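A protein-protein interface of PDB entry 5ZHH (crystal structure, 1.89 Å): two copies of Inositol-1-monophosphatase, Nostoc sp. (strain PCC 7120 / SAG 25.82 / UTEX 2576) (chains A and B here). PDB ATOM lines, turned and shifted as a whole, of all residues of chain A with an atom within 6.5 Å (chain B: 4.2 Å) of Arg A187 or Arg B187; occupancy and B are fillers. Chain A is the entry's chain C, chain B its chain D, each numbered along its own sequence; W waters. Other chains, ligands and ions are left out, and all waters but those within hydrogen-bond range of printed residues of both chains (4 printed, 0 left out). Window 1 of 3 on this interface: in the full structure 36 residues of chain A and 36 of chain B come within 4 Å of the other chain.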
ATOM      1  N   TYR A  99       7.326 -16.720 -31.414  1.00  0.00           N
ATOM      2  CA  TYR A  99       8.705 -16.896 -30.976  1.00  0.00           C
ATOM      3  C   TYR A  99       9.605 -16.819 -32.202  1.00  0.00           C
ATOM      4  O   TYR A  99       9.393 -17.573 -33.162  1.00  0.00           O
ATOM      5  CB  TYR A  99       8.873 -18.244 -30.260  1.00  0.00           C
ATOM      6  CG  TYR A  99      10.171 -18.362 -29.495  1.00  0.00           C
ATOM      7  CD1 TYR A  99      10.276 -17.899 -28.190  1.00  0.00           C
ATOM      8  CD2 TYR A  99      11.308 -18.891 -30.094  1.00  0.00           C
ATOM      9  CE1 TYR A  99      11.476 -17.991 -27.492  1.00  0.00           C
ATOM     10  CE2 TYR A  99      12.504 -18.990 -29.403  1.00  0.00           C
ATOM     11  CZ  TYR A  99      12.582 -18.536 -28.107  1.00  0.00           C
ATOM     12  OH  TYR A  99      13.779 -18.625 -27.421  1.00  0.00           O
ATOM     13  N   LEU A 156      26.297 -26.140 -28.594  1.00  0.00           N
ATOM     14  CA  LEU A 156      25.523 -27.077 -29.388  1.00  0.00           C
ATOM     15  C   LEU A 156      24.054 -26.692 -29.347  1.00  0.00           C
ATOM     16  O   LEU A 156      23.637 -25.805 -28.600  1.00  0.00           O
ATOM     17  CB  LEU A 156      25.696 -28.517 -28.877  1.00  0.00           C
ATOM     18  CG  LEU A 156      27.143 -28.989 -28.732  1.00  0.00           C
ATOM     19  CD1 LEU A 156      27.203 -30.429 -28.206  1.00  0.00           C
ATOM     20  CD2 LEU A 156      27.865 -28.873 -30.063  1.00  0.00           C
ATOM     21  N   VAL A 157      23.262 -27.404 -30.145  1.00  0.00           N
ATOM     22  CA  VAL A 157      21.817 -27.216 -30.167  1.00  0.00           C
ATOM     23  C   VAL A 157      21.170 -28.559 -30.465  1.00  0.00           C
ATOM     24  O   VAL A 157      21.747 -29.407 -31.147  1.00  0.00           O
ATOM     25  CB  VAL A 157      21.418 -26.134 -31.202  1.00  0.00           C
ATOM     26  CG1 VAL A 157      21.910 -26.523 -32.597  1.00  0.00           C
ATOM     27  CG2 VAL A 157      19.912 -25.877 -31.182  1.00  0.00           C
ATOM     28  N   THR A 158      19.964 -28.754 -29.941  1.00  0.00           N
ATOM     29  CA  THR A 158      19.220 -29.981 -30.173  1.00  0.00           C
ATOM     30  C   THR A 158      17.735 -29.664 -30.065  1.00  0.00           C
ATOM     31  O   THR A 158      17.338 -28.521 -29.816  1.00  0.00           O
ATOM     32  CB  THR A 158      19.659 -31.091 -29.200  1.00  0.00           C
ATOM     33  OG1 THR A 158      19.115 -32.340 -29.633  1.00  0.00           O
ATOM     34  CG2 THR A 158      19.190 -30.808 -27.775  1.00  0.00           C
ATOM     35  N   GLY A 159      16.911 -30.684 -30.288  1.00  0.00           N
ATOM     36  CA  GLY A 159      15.472 -30.553 -30.205  1.00  0.00           C
ATOM     37  C   GLY A 159      14.867 -31.823 -29.638  1.00  0.00           C
ATOM     38  O   GLY A 159      15.577 -32.772 -29.319  1.00  0.00           O
ATOM     39  N   PHE A 160      13.541 -31.812 -29.500  1.00  0.00           N
ATOM     40  CA  PHE A 160      12.809 -32.897 -28.858  1.00  0.00           C
ATOM     41  C   PHE A 160      11.556 -33.199 -29.663  1.00  0.00           C
ATOM     42  O   PHE A 160      10.856 -32.274 -30.088  1.00  0.00           O
ATOM     43  CB  PHE A 160      12.487 -32.526 -27.406  1.00  0.00           C
ATOM     44  CG  PHE A 160      13.717 -32.182 -26.620  1.00  0.00           C
ATOM     45  CD1 PHE A 160      14.479 -33.190 -26.031  1.00  0.00           C
ATOM     46  CD2 PHE A 160      14.153 -30.868 -26.531  1.00  0.00           C
ATOM     47  CE1 PHE A 160      15.643 -32.875 -25.342  1.00  0.00           C
ATOM     48  CE2 PHE A 160      15.311 -30.544 -25.850  1.00  0.00           C
ATOM     49  CZ  PHE A 160      16.059 -31.549 -25.249  1.00  0.00           C
ATOM     50  N   ALA A 161      11.304 -34.488 -29.897  1.00  0.00           N
ATOM     51  CA  ALA A 161      10.323 -34.917 -30.883  1.00  0.00           C
ATOM     52  C   ALA A 161       8.899 -34.886 -30.332  1.00  0.00           C
ATOM     53  O   ALA A 161       8.660 -34.905 -29.121  1.00  0.00           O
ATOM     54  CB  ALA A 161      10.658 -36.327 -31.377  1.00  0.00           C
ATOM     55  N   PHE A 175      20.614 -34.537 -23.899  1.00  0.00           N
ATOM     56  CA  PHE A 175      20.624 -33.112 -23.584  1.00  0.00           C
ATOM     57  C   PHE A 175      21.359 -32.834 -22.275  1.00  0.00           C
ATOM     58  O   PHE A 175      22.162 -31.898 -22.188  1.00  0.00           O
ATOM     59  CB  PHE A 175      19.189 -32.580 -23.516  1.00  0.00           C
ATOM     60  CG  PHE A 175      19.100 -31.143 -23.088  1.00  0.00           C
ATOM     61  CD1 PHE A 175      19.221 -30.125 -24.019  1.00  0.00           C
ATOM     62  CD2 PHE A 175      18.896 -30.808 -21.755  1.00  0.00           C
ATOM     63  CE1 PHE A 175      19.152 -28.804 -23.638  1.00  0.00           C
ATOM     64  CE2 PHE A 175      18.824 -29.479 -21.368  1.00  0.00           C
ATOM     65  CZ  PHE A 175      18.949 -28.479 -22.312  1.00  0.00           C
ATOM     66  N   GLN A 183      29.744 -25.880 -23.287  1.00  0.00           N
ATOM     67  CA  GLN A 183      29.428 -24.569 -22.789  1.00  0.00           C
ATOM     68  C   GLN A 183      27.906 -24.357 -22.748  1.00  0.00           C
ATOM     69  O   GLN A 183      27.455 -23.447 -22.170  1.00  0.00           O
ATOM     70  CB  GLN A 183      30.063 -23.488 -23.636  1.00  0.00           C
ATOM     71  CG  GLN A 183      31.559 -23.358 -23.483  1.00  0.00           C
ATOM     72  CD  GLN A 183      32.182 -22.292 -24.339  1.00  0.00           C
ATOM     73  OE1 GLN A 183      31.617 -21.805 -25.252  1.00  0.00           O
ATOM     74  NE2 GLN A 183      33.376 -21.984 -24.043  1.00  0.00           N
ATOM     75  N   GLY A 184      27.144 -25.210 -23.397  1.00  0.00           N
ATOM     76  CA  GLY A 184      25.697 -25.113 -23.386  1.00  0.00           C
ATOM     77  C   GLY A 184      25.092 -25.782 -24.601  1.00  0.00           C
ATOM     78  O   GLY A 184      25.733 -25.991 -25.630  1.00  0.00           O
ATOM     79  N   VAL A 185      23.829 -26.174 -24.456  1.00  0.00           N
ATOM     80  CA  VAL A 185      23.042 -26.744 -25.540  1.00  0.00           C
ATOM     81  C   VAL A 185      21.805 -25.878 -25.687  1.00  0.00           C
ATOM     82  O   VAL A 185      20.994 -25.778 -24.755  1.00  0.00           O
ATOM     83  CB  VAL A 185      22.659 -28.208 -25.278  1.00  0.00           C
ATOM     84  CG1 VAL A 185      21.906 -28.771 -26.481  1.00  0.00           C
ATOM     85  CG2 VAL A 185      23.904 -29.025 -24.977  1.00  0.00           C
ATOM     86  N   ARG A 186      21.675 -25.233 -26.836  1.00  0.00           N
ATOM     87  CA  ARG A 186      20.532 -24.384 -27.103  1.00  0.00           C
ATOM     88  C   ARG A 186      19.328 -25.211 -27.550  1.00  0.00           C
ATOM     89  O   ARG A 186      19.447 -26.371 -27.954  1.00  0.00           O
ATOM     90  CB  ARG A 186      20.894 -23.347 -28.167  1.00  0.00           C
ATOM     91  CG  ARG A 186      22.062 -22.440 -27.774  1.00  0.00           C
ATOM     92  CD  ARG A 186      21.635 -21.470 -26.669  1.00  0.00           C
ATOM     93  NE  ARG A 186      22.727 -20.663 -26.130  1.00  0.00           N
ATOM     94  CZ  ARG A 186      23.409 -20.965 -25.027  1.00  0.00           C
ATOM     95  NH1 ARG A 186      24.376 -20.160 -24.601  1.00  0.00           N
ATOM     96  NH2 ARG A 186      23.149 -22.092 -24.364  1.00  0.00           N
ATOM     97  N   ARG A 187      18.155 -24.583 -27.479  1.00  0.00           N
ATOM     98  CA  ARG A 187      16.899 -25.155 -27.976  1.00  0.00           C
ATOM     99  C   ARG A 187      16.147 -24.003 -28.629  1.00  0.00           C
ATOM    100  O   ARG A 187      15.558 -23.177 -27.929  1.00  0.00           O
ATOM    101  CB  ARG A 187      16.086 -25.779 -26.844  1.00  0.00           C
ATOM    102  CG  ARG A 187      15.002 -26.816 -27.210  1.00  0.00           C
ATOM    103  CD  ARG A 187      14.571 -26.806 -28.657  1.00  0.00           C
ATOM    104  NE  ARG A 187      13.409 -27.657 -28.921  1.00  0.00           N
ATOM    105  CZ  ARG A 187      13.088 -28.104 -30.133  1.00  0.00           C
ATOM    106  NH1 ARG A 187      13.853 -27.795 -31.173  1.00  0.00           N
ATOM    107  NH2 ARG A 187      12.022 -28.875 -30.311  1.00  0.00           N
ATOM    108  N   SER A 188      16.165 -23.964 -29.959  1.00  0.00           N
ATOM    109  CA  SER A 188      15.566 -22.874 -30.718  1.00  0.00           C
ATOM    110  C   SER A 188      14.138 -23.176 -31.154  1.00  0.00           C
ATOM    111  O   SER A 188      13.302 -22.267 -31.191  1.00  0.00           O
ATOM    112  CB  SER A 188      16.417 -22.570 -31.954  1.00  0.00           C
ATOM    113  OG  SER A 188      16.217 -23.579 -32.941  1.00  0.00           O
ATOM    114  N   GLY A 189      13.843 -24.434 -31.484  1.00  0.00           N
ATOM    115  CA  GLY A 189      12.541 -24.812 -31.990  1.00  0.00           C
ATOM    116  C   GLY A 189      12.420 -24.909 -33.498  1.00  0.00           C
ATOM    117  O   GLY A 189      11.308 -25.137 -33.994  1.00  0.00           O
ATOM    118  N   SER A 190      13.518 -24.756 -34.241  1.00  0.00           N
ATOM    119  CA  SER A 190      13.502 -24.914 -35.695  1.00  0.00           C
ATOM    120  C   SER A 190      14.733 -25.698 -36.124  1.00  0.00           C
ATOM    121  O   SER A 190      15.851 -25.172 -36.064  1.00  0.00           O
ATOM    122  CB  SER A 190      13.457 -23.556 -36.399  1.00  0.00           C
ATOM    123  OG  SER A 190      13.702 -23.714 -37.785  1.00  0.00           O
ATOM    124  N   ALA A 191      14.519 -26.930 -36.601  1.00  0.00           N
ATOM    125  CA  ALA A 191      15.629 -27.779 -37.028  1.00  0.00           C
ATOM    126  C   ALA A 191      16.350 -27.197 -38.235  1.00  0.00           C
ATOM    127  O   ALA A 191      17.579 -27.294 -38.338  1.00  0.00           O
ATOM    128  CB  ALA A 191      15.123 -29.188 -37.348  1.00  0.00           C
ATOM    129  N   ASP A 194      18.486 -24.490 -37.015  1.00  0.00           N
ATOM    130  CA  ASP A 194      19.611 -25.066 -36.286  1.00  0.00           C
ATOM    131  C   ASP A 194      20.707 -25.513 -37.246  1.00  0.00           C
ATOM    132  O   ASP A 194      21.892 -25.255 -37.014  1.00  0.00           O
ATOM    133  CB  ASP A 194      19.136 -26.232 -35.409  1.00  0.00           C
ATOM    134  CG  ASP A 194      18.240 -25.776 -34.261  1.00  0.00           C
ATOM    135  OD1 ASP A 194      18.306 -24.581 -33.887  1.00  0.00           O
ATOM    136  OD2 ASP A 194      17.486 -26.615 -33.712  1.00  0.00           O
ATOM    137  N   GLU A 208      19.597 -34.432 -33.375  1.00  0.00           N
ATOM    138  CA  GLU A 208      18.185 -34.568 -33.043  1.00  0.00           C
ATOM    139  C   GLU A 208      17.676 -35.903 -33.567  1.00  0.00           C
ATOM    140  O   GLU A 208      18.182 -36.425 -34.568  1.00  0.00           O
ATOM    141  CB  GLU A 208      17.355 -33.409 -33.622  1.00  0.00           C
ATOM    142  CG  GLU A 208      15.932 -33.352 -33.101  1.00  0.00           C
ATOM    143  CD  GLU A 208      15.253 -32.006 -33.352  1.00  0.00           C
ATOM    144  OE1 GLU A 208      14.147 -31.806 -32.800  1.00  0.00           O
ATOM    145  OE2 GLU A 208      15.822 -31.153 -34.085  1.00  0.00           O
ATOM    146  N   THR B 158      14.009 -21.687 -20.174  1.00  0.00           N
ATOM    147  CA  THR B 158      14.783 -21.793 -18.944  1.00  0.00           C
ATOM    148  C   THR B 158      16.265 -21.748 -19.303  1.00  0.00           C
ATOM    149  O   THR B 158      16.638 -21.669 -20.474  1.00  0.00           O
ATOM    150  CB  THR B 158      14.412 -23.076 -18.166  1.00  0.00           C
ATOM    151  OG1 THR B 158      14.962 -23.021 -16.845  1.00  0.00           O
ATOM    152  CG2 THR B 158      14.933 -24.319 -18.879  1.00  0.00           C
ATOM    153  N   GLY B 159      17.114 -21.785 -18.274  1.00  0.00           N
ATOM    154  CA  GLY B 159      18.551 -21.792 -18.457  1.00  0.00           C
ATOM    155  C   GLY B 159      19.219 -22.671 -17.418  1.00  0.00           C
ATOM    156  O   GLY B 159      18.562 -23.219 -16.529  1.00  0.00           O
ATOM    157  N   PHE B 160      20.545 -22.785 -17.536  1.00  0.00           N
ATOM    158  CA  PHE B 160      21.324 -23.698 -16.708  1.00  0.00           C
ATOM    159  C   PHE B 160      22.575 -22.986 -16.226  1.00  0.00           C
ATOM    160  O   PHE B 160      23.266 -22.337 -17.016  1.00  0.00           O
ATOM    161  CB  PHE B 160      21.660 -24.966 -17.497  1.00  0.00           C
ATOM    162  CG  PHE B 160      20.441 -25.633 -18.057  1.00  0.00           C
ATOM    163  CD1 PHE B 160      19.690 -26.504 -17.274  1.00  0.00           C
ATOM    164  CD2 PHE B 160      20.010 -25.349 -19.342  1.00  0.00           C
ATOM    165  CE1 PHE B 160      18.541 -27.097 -17.783  1.00  0.00           C
ATOM    166  CE2 PHE B 160      18.867 -25.939 -19.856  1.00  0.00           C
ATOM    167  CZ  PHE B 160      18.133 -26.820 -19.073  1.00  0.00           C
ATOM    168  N   VAL B 185      10.220 -26.349 -24.169  1.00  0.00           N
ATOM    169  CA  VAL B 185      10.994 -25.440 -23.336  1.00  0.00           C
ATOM    170  C   VAL B 185      12.193 -24.993 -24.158  1.00  0.00           C
ATOM    171  O   VAL B 185      13.018 -25.820 -24.568  1.00  0.00           O
ATOM    172  CB  VAL B 185      11.445 -26.078 -22.014  1.00  0.00           C
ATOM    173  CG1 VAL B 185      12.191 -25.034 -21.169  1.00  0.00           C
ATOM    174  CG2 VAL B 185      10.248 -26.635 -21.253  1.00  0.00           C
ATOM    175  N   ARG B 186      12.258 -23.703 -24.442  1.00  0.00           N
ATOM    176  CA  ARG B 186      13.375 -23.167 -25.193  1.00  0.00           C
ATOM    177  C   ARG B 186      14.580 -22.952 -24.278  1.00  0.00           C
ATOM    178  O   ARG B 186      14.472 -22.948 -23.050  1.00  0.00           O
ATOM    179  CB  ARG B 186      12.964 -21.856 -25.858  1.00  0.00           C
ATOM    180  CG  ARG B 186      11.782 -22.003 -26.825  1.00  0.00           C
ATOM    181  CD  ARG B 186      12.214 -22.764 -28.069  1.00  0.00           C
ATOM    182  NE  ARG B 186      11.102 -23.087 -28.970  1.00  0.00           N
ATOM    183  CZ  ARG B 186      10.460 -24.256 -28.982  1.00  0.00           C
ATOM    184  NH1 ARG B 186       9.468 -24.469 -29.847  1.00  0.00           N
ATOM    185  NH2 ARG B 186      10.793 -25.215 -28.119  1.00  0.00           N
ATOM    186  N   ARG B 187      15.747 -22.794 -24.898  1.00  0.00           N
ATOM    187  CA  ARG B 187      16.963 -22.385 -24.197  1.00  0.00           C
ATOM    188  C   ARG B 187      17.682 -21.431 -25.143  1.00  0.00           C
ATOM    189  O   ARG B 187      18.283 -21.864 -26.129  1.00  0.00           O
ATOM    190  CB  ARG B 187      17.834 -23.576 -23.817  1.00  0.00           C
ATOM    191  CG  ARG B 187      18.771 -23.331 -22.617  1.00  0.00           C
ATOM    192  CD  ARG B 187      19.811 -22.259 -22.878  1.00  0.00           C
ATOM    193  NE  ARG B 187      20.815 -22.139 -21.820  1.00  0.00           N
ATOM    194  CZ  ARG B 187      20.887 -21.132 -20.946  1.00  0.00           C
ATOM    195  NH1 ARG B 187      20.004 -20.132 -20.976  1.00  0.00           N
ATOM    196  NH2 ARG B 187      21.858 -21.117 -20.036  1.00  0.00           N
ATOM    197  N   SER B 188      17.608 -20.138 -24.836  1.00  0.00           N
ATOM    198  CA  SER B 188      18.165 -19.091 -25.685  1.00  0.00           C
ATOM    199  C   SER B 188      19.593 -18.721 -25.314  1.00  0.00           C
ATOM    200  O   SER B 188      20.393 -18.400 -26.203  1.00  0.00           O
ATOM    201  CB  SER B 188      17.313 -17.829 -25.582  1.00  0.00           C
ATOM    202  OG  SER B 188      17.566 -17.189 -24.336  1.00  0.00           O
ATOM    203  N   GLY B 189      19.924 -18.760 -24.030  1.00  0.00           N
ATOM    204  CA  GLY B 189      21.230 -18.360 -23.557  1.00  0.00           C
ATOM    205  C   GLY B 189      21.331 -16.948 -23.022  1.00  0.00           C
ATOM    206  O   GLY B 189      22.446 -16.508 -22.715  1.00  0.00           O
HETATM  207  O   HOH W   1      11.286 -28.235 -27.138  1.00  0.00           O
HETATM  208  O   HOH W   2       8.761 -24.486 -33.139  1.00  0.00           O
HETATM  209  O   HOH W   3      22.850 -23.993 -21.613  1.00  0.00           O
HETATM  210  O   HOH W   4      24.926 -17.061 -23.647  1.00  0.00           O
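Hydrophobic or aromatic side chains of chain A that line the printed part of chain B: Tyr A99 and Phe A175. Of the 8 printed residues of chain B, 6 touch a printed residue of chain A. Hydrophobic or aromatic side chains of chain B within 4 Å of the printed part of chain A: Phe B160. Among the printed residues, 11 pairs touch across the chains. Among the printed residues, no Asp or Glu carboxylate lies within 4 Å of a Lys or Arg side-chain nitrogen of the other chain.
Val A185 touches Arg B187, and with the chains exchanged Arg A187 touches Val B185. Arg A186 touches Ser B188, and with the chains exchanged Ser A188 touches Arg B186. Arg A186 touches Gly B189, and with the chains exchanged Gly A189 touches Arg B186. Arg A187 touches its own counterpart, Arg B187. 8 positions are printed for both chains. Of the 11 pairs that touch across the chains among the printed residues, 9 have their exchanged pair printed and touching as well.
The backbone NH (N) of Arg A186 is in hydrogen-bond range of the backbone carbonyl oxygen (O) of Leu A156. N of Thr A158 is in hydrogen-bond range of O of Arg A186, at 3.1 Å. The side-chain hydroxyl of Ser A188 lies within hydrogen-bond range of the backbone NH of Ser A190 (3.2 Å). The side-chain hydroxyl (OG) of Ser A188 sits at hydrogen-bond distance from the side-chain carboxylate (OD1) of Asp A194. The backbone NH (N) of Thr B158 sits at hydrogen-bond distance from the backbone carbonyl oxygen (O) of Arg B186 (3.2 Å).
The guanidinium group (NE) of Arg A186 lies within hydrogen-bond range of the backbone carbonyl oxygen (O) of Ser B188, 3.3 Å away. N of Arg A187 lies within hydrogen-bond range of O of Arg B187 (3.0 Å). O of Ser A188 lies within hydrogen-bond range of NE of Arg B186 (3.2 Å). The guanidinium group of Arg A186 sits close to the guanidinium group of Arg B187, 3.5 Å away.
Water W4 lies within hydrogen-bond range of O of Gly B189 and NH1 of Arg A186. Water W3 bridges the guanidinium group of Arg B187 (2.8 Å) and the guanidinium group of Arg A186 (3.4 Å). Water W2 bridges O of Gly A189 (2.8 Å) and NH1 of Arg B186 (3.4 Å). Water W1 lies within hydrogen-bond range of NE of Arg A187 (2.8 Å) and NH2 of Arg B186 (3.2 Å).
Among the printed residues, merely in contact across the chains: Tyr A99 with Arg B186, Phe A175 with Phe B160, Val A185 with Arg B187, Arg A186 with Gly B189, Arg A187 with Val B185, Arg A187 with Arg B186 and Gly A189 with Arg B186.
Arg A187 touches three residues of chain B. Arg B187 touches just these residues of chain A: Val A185 (3.9 Å), Arg A186 (3.4 Å) and Arg A187 (3.0 Å). Of the printed residues of chain B, Tyr A99 touches Arg B186 (3.7 Å). Of the printed residues of chain A, Val B185 touches Arg A187 (3.5 Å). Leu A156 touches none of the printed residues of chain B. The nearest printed residue of chain A that does not touch Val B185 is Phe A160 (5.4 Å).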
